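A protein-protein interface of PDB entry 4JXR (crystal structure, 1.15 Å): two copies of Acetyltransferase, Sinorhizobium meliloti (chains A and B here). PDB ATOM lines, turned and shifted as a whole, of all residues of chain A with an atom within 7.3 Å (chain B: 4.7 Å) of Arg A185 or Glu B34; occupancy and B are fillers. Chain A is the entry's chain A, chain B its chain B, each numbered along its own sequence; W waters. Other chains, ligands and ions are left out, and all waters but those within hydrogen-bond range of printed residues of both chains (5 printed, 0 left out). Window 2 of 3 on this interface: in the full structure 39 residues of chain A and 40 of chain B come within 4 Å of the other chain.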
ATOM      1  N   ARG A  78     -17.068 -14.199  12.463  1.00  0.00           N
ATOM      2  CA  ARG A  78     -17.060 -12.952  11.712  1.00  0.00           C
ATOM      3  C   ARG A  78     -15.602 -12.556  11.501  1.00  0.00           C
ATOM      4  O   ARG A  78     -14.712 -12.815  12.328  1.00  0.00           O
ATOM      5  CB  ARG A  78     -17.830 -11.821  12.368  1.00  0.00           C
ATOM      6  CG  ARG A  78     -19.357 -12.008  12.616  1.00  0.00           C
ATOM      7  CD  ARG A  78     -20.127 -12.740  11.510  1.00  0.00           C
ATOM      8  NE  ARG A  78     -21.600 -12.598  11.618  1.00  0.00           N
ATOM      9  CZ  ARG A  78     -22.475 -13.122  10.762  1.00  0.00           C
ATOM     10  NH1 ARG A  78     -23.788 -12.928  10.923  1.00  0.00           N
ATOM     11  NH2 ARG A  78     -22.058 -13.863   9.749  1.00  0.00           N
ATOM     12  N   THR A  79     -15.375 -11.948  10.343  1.00  0.00           N
ATOM     13  CA  THR A  79     -14.058 -11.640   9.851  1.00  0.00           C
ATOM     14  C   THR A  79     -13.125 -11.052  10.893  1.00  0.00           C
ATOM     15  O   THR A  79     -11.984 -11.505  11.056  1.00  0.00           O
ATOM     16  CB  THR A  79     -14.145 -10.722   8.629  1.00  0.00           C
ATOM     17  OG1 THR A  79     -15.045 -11.258   7.690  1.00  0.00           O
ATOM     18  CG2 THR A  79     -12.764 -10.518   8.014  1.00  0.00           C
ATOM     19  N   ALA A  80     -13.554  -9.997  11.581  1.00  0.00           N
ATOM     20  CA  ALA A  80     -12.640  -9.311  12.469  1.00  0.00           C
ATOM     21  C   ALA A  80     -12.226 -10.131  13.669  1.00  0.00           C
ATOM     22  O   ALA A  80     -11.260  -9.789  14.304  1.00  0.00           O
ATOM     23  CB  ALA A  80     -13.159  -7.960  12.858  1.00  0.00           C
ATOM     24  N   ARG A  82     -11.122 -13.189  13.458  1.00  0.00           N
ATOM     25  CA  ARG A  82     -10.400 -14.372  12.988  1.00  0.00           C
ATOM     26  C   ARG A  82      -9.153 -14.717  13.788  1.00  0.00           C
ATOM     27  O   ARG A  82      -8.736 -15.886  13.760  1.00  0.00           O
ATOM     28  CB  ARG A  82     -10.076 -14.249  11.495  1.00  0.00           C
ATOM     29  CG  ARG A  82      -9.123 -13.119  11.125  1.00  0.00           C
ATOM     30  CD  ARG A  82      -9.214 -12.851   9.627  1.00  0.00           C
ATOM     31  NE  ARG A  82      -8.350 -11.774   9.149  1.00  0.00           N
ATOM     32  CZ  ARG A  82      -8.609 -10.478   9.270  1.00  0.00           C
ATOM     33  NH1 ARG A  82      -9.710 -10.063   9.863  1.00  0.00           N
ATOM     34  NH2 ARG A  82      -7.758  -9.588   8.759  1.00  0.00           N
ATOM     35  N   PHE A  83      -8.553 -13.777  14.481  1.00  0.00           N
ATOM     36  CA  PHE A  83      -7.370 -14.041  15.307  1.00  0.00           C
ATOM     37  C   PHE A  83      -7.716 -14.444  16.731  1.00  0.00           C
ATOM     38  O   PHE A  83      -6.808 -14.655  17.546  1.00  0.00           O
ATOM     39  CB  PHE A  83      -6.429 -12.825  15.324  1.00  0.00           C
ATOM     40  CG  PHE A  83      -5.994 -12.452  13.935  1.00  0.00           C
ATOM     41  CD1 PHE A  83      -5.067 -13.183  13.256  1.00  0.00           C
ATOM     42  CD2 PHE A  83      -6.584 -11.371  13.291  1.00  0.00           C
ATOM     43  CE1 PHE A  83      -4.752 -12.849  11.922  1.00  0.00           C
ATOM     44  CE2 PHE A  83      -6.262 -11.054  11.975  1.00  0.00           C
ATOM     45  CZ  PHE A  83      -5.355 -11.780  11.322  1.00  0.00           C
ATOM     46  N   GLU A 176      -0.330 -10.509   6.706  1.00  0.00           N
ATOM     47  CA  GLU A 176      -1.373 -10.652   5.723  1.00  0.00           C
ATOM     48  C   GLU A 176      -1.182 -11.900   4.907  1.00  0.00           C
ATOM     49  O   GLU A 176      -0.084 -12.224   4.460  1.00  0.00           O
ATOM     50  CB  GLU A 176      -1.494  -9.421   4.798  1.00  0.00           C
ATOM     51  CG  GLU A 176      -1.907  -8.156   5.514  1.00  0.00           C
ATOM     52  CD  GLU A 176      -1.976  -6.975   4.574  1.00  0.00           C
ATOM     53  OE1 GLU A 176      -1.873  -7.186   3.336  1.00  0.00           O
ATOM     54  OE2 GLU A 176      -2.130  -5.836   5.079  1.00  0.00           O
ATOM     55  N   GLY A 177      -2.273 -12.567   4.648  1.00  0.00           N
ATOM     56  CA  GLY A 177      -2.326 -13.638   3.686  1.00  0.00           C
ATOM     57  C   GLY A 177      -1.826 -14.982   4.131  1.00  0.00           C
ATOM     58  O   GLY A 177      -1.722 -15.881   3.322  1.00  0.00           O
ATOM     59  N   PRO A 180      -3.908 -17.444  10.407  1.00  0.00           N
ATOM     60  CA  PRO A 180      -5.384 -17.467  10.256  1.00  0.00           C
ATOM     61  C   PRO A 180      -5.956 -16.204   9.629  1.00  0.00           C
ATOM     62  O   PRO A 180      -7.177 -16.010   9.648  1.00  0.00           O
ATOM     63  CB  PRO A 180      -5.850 -17.663  11.708  1.00  0.00           C
ATOM     64  CG  PRO A 180      -4.830 -16.859  12.474  1.00  0.00           C
ATOM     65  CD  PRO A 180      -3.518 -17.115  11.771  1.00  0.00           C
ATOM     66  N   ASP A 181      -5.123 -15.338   9.034  1.00  0.00           N
ATOM     67  CA  ASP A 181      -5.644 -14.162   8.337  1.00  0.00           C
ATOM     68  C   ASP A 181      -6.576 -14.546   7.217  1.00  0.00           C
ATOM     69  O   ASP A 181      -7.414 -13.729   6.807  1.00  0.00           O
ATOM     70  CB  ASP A 181      -4.479 -13.347   7.751  1.00  0.00           C
ATOM     71  CG  ASP A 181      -4.922 -12.036   7.217  1.00  0.00           C
ATOM     72  OD1 ASP A 181      -5.574 -11.264   7.933  1.00  0.00           O
ATOM     73  OD2 ASP A 181      -4.595 -11.724   6.034  1.00  0.00           O
ATOM     74  N   THR A 182      -6.413 -15.742   6.691  1.00  0.00           N
ATOM     75  CA  THR A 182      -7.201 -16.254   5.593  1.00  0.00           C
ATOM     76  C   THR A 182      -8.595 -16.771   5.974  1.00  0.00           C
ATOM     77  O   THR A 182      -9.370 -17.137   5.103  1.00  0.00           O
ATOM     78  CB  THR A 182      -6.434 -17.375   4.907  1.00  0.00           C
ATOM     79  OG1 THR A 182      -6.043 -18.300   5.920  1.00  0.00           O
ATOM     80  CG2 THR A 182      -5.185 -16.843   4.248  1.00  0.00           C
ATOM     81  N   LEU A 183      -8.909 -16.839   7.287  1.00  0.00           N
ATOM     82  CA  LEU A 183     -10.229 -17.294   7.725  1.00  0.00           C
ATOM     83  C   LEU A 183     -11.254 -16.202   7.562  1.00  0.00           C
ATOM     84  O   LEU A 183     -11.029 -15.028   7.829  1.00  0.00           O
ATOM     85  CB  LEU A 183     -10.213 -17.691   9.197  1.00  0.00           C
ATOM     86  CG  LEU A 183      -9.629 -19.037   9.537  1.00  0.00           C
ATOM     87  CD1 LEU A 183      -9.504 -19.154  11.034  1.00  0.00           C
ATOM     88  CD2 LEU A 183     -10.508 -20.133   9.025  1.00  0.00           C
ATOM     89  N   TYR A 184     -12.452 -16.637   7.196  1.00  0.00           N
ATOM     90  CA  TYR A 184     -13.627 -15.782   7.208  1.00  0.00           C
ATOM     91  C   TYR A 184     -13.526 -14.589   6.289  1.00  0.00           C
ATOM     92  O   TYR A 184     -13.981 -13.508   6.610  1.00  0.00           O
ATOM     93  CB  TYR A 184     -14.030 -15.357   8.644  1.00  0.00           C
ATOM     94  CG  TYR A 184     -14.039 -16.552   9.599  1.00  0.00           C
ATOM     95  CD1 TYR A 184     -14.638 -17.763   9.271  1.00  0.00           C
ATOM     96  CD2 TYR A 184     -13.461 -16.464  10.828  1.00  0.00           C
ATOM     97  CE1 TYR A 184     -14.576 -18.857  10.114  1.00  0.00           C
ATOM     98  CE2 TYR A 184     -13.382 -17.540  11.697  1.00  0.00           C
ATOM     99  CZ  TYR A 184     -13.919 -18.738  11.314  1.00  0.00           C
ATOM    100  OH  TYR A 184     -13.867 -19.879  12.109  1.00  0.00           O
ATOM    101  N   ARG A 185     -12.912 -14.770   5.119  1.00  0.00           N
ATOM    102  CA  ARG A 185     -12.708 -13.711   4.137  1.00  0.00           C
ATOM    103  C   ARG A 185     -13.609 -14.013   2.942  1.00  0.00           C
ATOM    104  O   ARG A 185     -13.936 -15.161   2.682  1.00  0.00           O
ATOM    105  CB  ARG A 185     -11.254 -13.617   3.691  1.00  0.00           C
ATOM    106  CG  ARG A 185     -10.274 -13.632   4.820  1.00  0.00           C
ATOM    107  CD  ARG A 185     -10.442 -12.554   5.886  1.00  0.00           C
ATOM    108  NE  ARG A 185     -10.337 -11.187   5.406  1.00  0.00           N
ATOM    109  CZ  ARG A 185      -9.183 -10.565   5.294  1.00  0.00           C
ATOM    110  NH1 ARG A 185      -8.023 -11.141   5.579  1.00  0.00           N
ATOM    111  NH2 ARG A 185      -9.192  -9.300   4.906  1.00  0.00           N
ATOM    112  N   SER A 186     -14.016 -13.020   2.237  1.00  0.00           N
ATOM    113  CA  SER A 186     -14.979 -13.320   1.158  1.00  0.00           C
ATOM    114  C   SER A 186     -15.193 -12.076   0.307  1.00  0.00           C
ATOM    115  O   SER A 186     -16.022 -12.051  -0.610  1.00  0.00           O
ATOM    116  CB  SER A 186     -16.306 -13.904   1.722  1.00  0.00           C
ATOM    117  OG  SER A 186     -17.063 -12.960   2.471  1.00  0.00           O
ATOM    118  OXT SER A 186     -14.495 -11.081   0.541  1.00  0.00           O
ATOM    119  N   VAL B  25     -20.773  -1.969   7.852  1.00  0.00           N
ATOM    120  CA  VAL B  25     -19.793  -2.960   7.538  1.00  0.00           C
ATOM    121  C   VAL B  25     -18.524  -2.335   6.971  1.00  0.00           C
ATOM    122  O   VAL B  25     -17.408  -2.706   7.346  1.00  0.00           O
ATOM    123  CB  VAL B  25     -20.374  -4.013   6.589  1.00  0.00           C
ATOM    124  CG1 VAL B  25     -19.265  -4.912   6.041  1.00  0.00           C
ATOM    125  CG2 VAL B  25     -21.436  -4.869   7.305  1.00  0.00           C
ATOM    126  N   LEU B  26     -18.701  -1.445   6.025  1.00  0.00           N
ATOM    127  CA  LEU B  26     -17.564  -0.869   5.329  1.00  0.00           C
ATOM    128  C   LEU B  26     -16.841   0.163   6.184  1.00  0.00           C
ATOM    129  O   LEU B  26     -15.599   0.215   6.099  1.00  0.00           O
ATOM    130  CB  LEU B  26     -18.049  -0.212   4.019  1.00  0.00           C
ATOM    131  CG  LEU B  26     -18.579  -1.194   2.973  1.00  0.00           C
ATOM    132  CD1 LEU B  26     -19.128  -0.419   1.812  1.00  0.00           C
ATOM    133  CD2 LEU B  26     -17.531  -2.185   2.557  1.00  0.00           C
ATOM    134  N   TYR B  32     -18.249  -6.687  13.065  1.00  0.00           N
ATOM    135  CA  TYR B  32     -16.963  -7.318  12.729  1.00  0.00           C
ATOM    136  C   TYR B  32     -17.066  -8.075  11.425  1.00  0.00           C
ATOM    137  O   TYR B  32     -16.128  -8.681  11.007  1.00  0.00           O
ATOM    138  CB  TYR B  32     -16.508  -8.223  13.870  1.00  0.00           C
ATOM    139  CG  TYR B  32     -15.956  -7.427  15.064  1.00  0.00           C
ATOM    140  CD1 TYR B  32     -16.006  -6.009  15.144  1.00  0.00           C
ATOM    141  CD2 TYR B  32     -15.385  -8.109  16.127  1.00  0.00           C
ATOM    142  CE1 TYR B  32     -15.518  -5.344  16.255  1.00  0.00           C
ATOM    143  CE2 TYR B  32     -14.913  -7.465  17.244  1.00  0.00           C
ATOM    144  CZ  TYR B  32     -14.985  -6.079  17.313  1.00  0.00           C
ATOM    145  OH  TYR B  32     -14.492  -5.412  18.421  1.00  0.00           O
ATOM    146  N   GLU B  33     -18.263  -8.070  10.856  1.00  0.00           N
ATOM    147  CA  GLU B  33     -18.227  -8.460   9.380  1.00  0.00           C
ATOM    148  C   GLU B  33     -17.498  -7.480   8.366  1.00  0.00           C
ATOM    149  O   GLU B  33     -17.406  -6.292   8.639  1.00  0.00           O
ATOM    150  CB  GLU B  33     -19.653  -8.628   8.864  1.00  0.00           C
ATOM    151  CG  GLU B  33     -20.449  -9.764   9.477  1.00  0.00           C
ATOM    152  CD  GLU B  33     -21.734 -10.039   8.712  1.00  0.00           C
ATOM    153  OE1 GLU B  33     -22.725  -9.338   8.946  1.00  0.00           O
ATOM    154  OE2 GLU B  33     -21.748 -10.942   7.866  1.00  0.00           O
ATOM    155  N   GLU B  34     -16.820  -8.090   7.407  1.00  0.00           N
ATOM    156  CA  GLU B  34     -16.035  -7.345   6.458  1.00  0.00           C
ATOM    157  C   GLU B  34     -16.714  -7.114   5.102  1.00  0.00           C
ATOM    158  O   GLU B  34     -16.562  -6.076   4.543  1.00  0.00           O
ATOM    159  CB  GLU B  34     -14.700  -8.061   6.238  1.00  0.00           C
ATOM    160  CG  GLU B  34     -13.876  -7.559   5.064  1.00  0.00           C
ATOM    161  CD  GLU B  34     -12.600  -8.393   4.859  1.00  0.00           C
ATOM    162  OE1 GLU B  34     -12.673  -9.594   4.588  1.00  0.00           O
ATOM    163  OE2 GLU B  34     -11.573  -7.776   5.005  1.00  0.00           O
ATOM    164  N   THR B  35     -17.456  -8.093   4.623  1.00  0.00           N
ATOM    165  CA  THR B  35     -18.084  -8.029   3.335  1.00  0.00           C
ATOM    166  C   THR B  35     -19.570  -7.791   3.557  1.00  0.00           C
ATOM    167  O   THR B  35     -20.242  -8.512   4.261  1.00  0.00           O
ATOM    168  CB  THR B  35     -17.895  -9.345   2.565  1.00  0.00           C
ATOM    169  OG1 THR B  35     -16.507  -9.537   2.369  1.00  0.00           O
ATOM    170  CG2 THR B  35     -18.571  -9.294   1.196  1.00  0.00           C
ATOM    171  N   PRO B  36     -20.123  -6.719   2.964  1.00  0.00           N
ATOM    172  CA  PRO B  36     -21.556  -6.464   3.156  1.00  0.00           C
ATOM    173  C   PRO B  36     -22.396  -7.630   2.700  1.00  0.00           C
ATOM    174  O   PRO B  36     -22.258  -8.074   1.561  1.00  0.00           O
ATOM    175  CB  PRO B  36     -21.820  -5.209   2.314  1.00  0.00           C
ATOM    176  CG  PRO B  36     -20.479  -4.506   2.308  1.00  0.00           C
ATOM    177  CD  PRO B  36     -19.496  -5.632   2.209  1.00  0.00           C
HETATM  178  O   HOH W   1     -20.187 -13.282   8.362  1.00  0.00           O
HETATM  179  O   HOH W   2     -15.124  -7.734   0.837  1.00  0.00           O
HETATM  180  O   HOH W   3     -11.668 -10.295   2.085  1.00  0.00           O
HETATM  181  O   HOH W   4     -14.959 -10.917   4.112  1.00  0.00           O
HETATM  182  O   HOH W   5     -17.682 -10.689   6.066  1.00  0.00           O
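O of Tyr B32 lies within hydrogen-bond range of N of Ala A80, 2.9 Å away.
The backbone carbonyl oxygen (O) of Tyr B32 sits at hydrogen-bond distance from the backbone NH (N) of Thr A79, at 3.4 Å.
The chain-end carboxylate (OXT) of Ser A186 lies within hydrogen-bond range of the side-chain hydroxyl (OG1) of Thr B35 (3.1 Å).
The side-chain carboxylate (OE2) of Glu B34 lies within salt-bridge range of the guanidinium group (NH2) of Arg A185 (2.8 Å).
NH2 of Arg A78 lies within salt-bridge range of OE2 of Glu B33 (3.5 Å).
OD1 of Asp A181 lies within salt-bridge range of NH1 of Arg A185 (3.4 Å).
O of Tyr A184 sits at hydrogen-bond distance from OG1 of Thr A79 (2.7 Å).
The backbone carbonyl oxygen (O) of Thr A79 sits at hydrogen-bond distance from the guanidinium group (NH1) of Arg A82 (2.9 Å).
Among the printed residues, merely in contact across the chains: Thr A79 with Glu B34 (3.5 Å) and Arg A78 with Tyr B32 (3.8 Å).
Arg A185 touches one residue of chain B.
Of chain A, only Thr A79 and Arg A185 come within 4 Å of Glu B34.
Printed residues of chain B within 4 Å of Arg A78: Tyr B32 (3.8 Å) and Glu B33 (3.5 Å).
Printed residues of chain A within 4 Å of Thr B35: Ser A186 (3.1 Å).
Of the printed residues of chain B, Thr A79 touches Tyr B32 (3.4 Å) and Glu B34 (3.5 Å).
Printed residues of chain B within 4 Å of Ser A186: Thr B35.
Of the 14 printed residues of chain A, 5 touch a printed residue of chain B.
Hydrophobic or aromatic side chains of chain A that line the printed part of chain B: Ala A80.
Of the 7 printed residues of chain B, 4 touch a printed residue of chain A.
Hydrophobic or aromatic side chains of chain B within 4 Å of the printed part of chain A: Tyr B32.
Among the printed residues, 7 pairs touch across the chains.
No position is printed for both chains.
Water W1 bridges NH2 of Arg A78 and OE2 of Glu B33.
Water W4 lies within hydrogen-bond range of the side-chain carboxylate (OE1) of Glu B34, the side-chain hydroxyl (OG1) of Thr B35 and the backbone NH (N) of Ser A186.
Water W2 bridges the side-chain hydroxyl of Thr B35 and the chain-end carboxylate of Ser A186.
Water W3 bridges OE1 of Glu B34 (2.8 Å) and OXT of Ser A186 (3.3 Å).
Water W5 lies within hydrogen-bond range of N of Thr B35 (3.0 Å), N of Glu B34 (3.0 Å) and OG1 of Thr A79 (3.1 Å).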
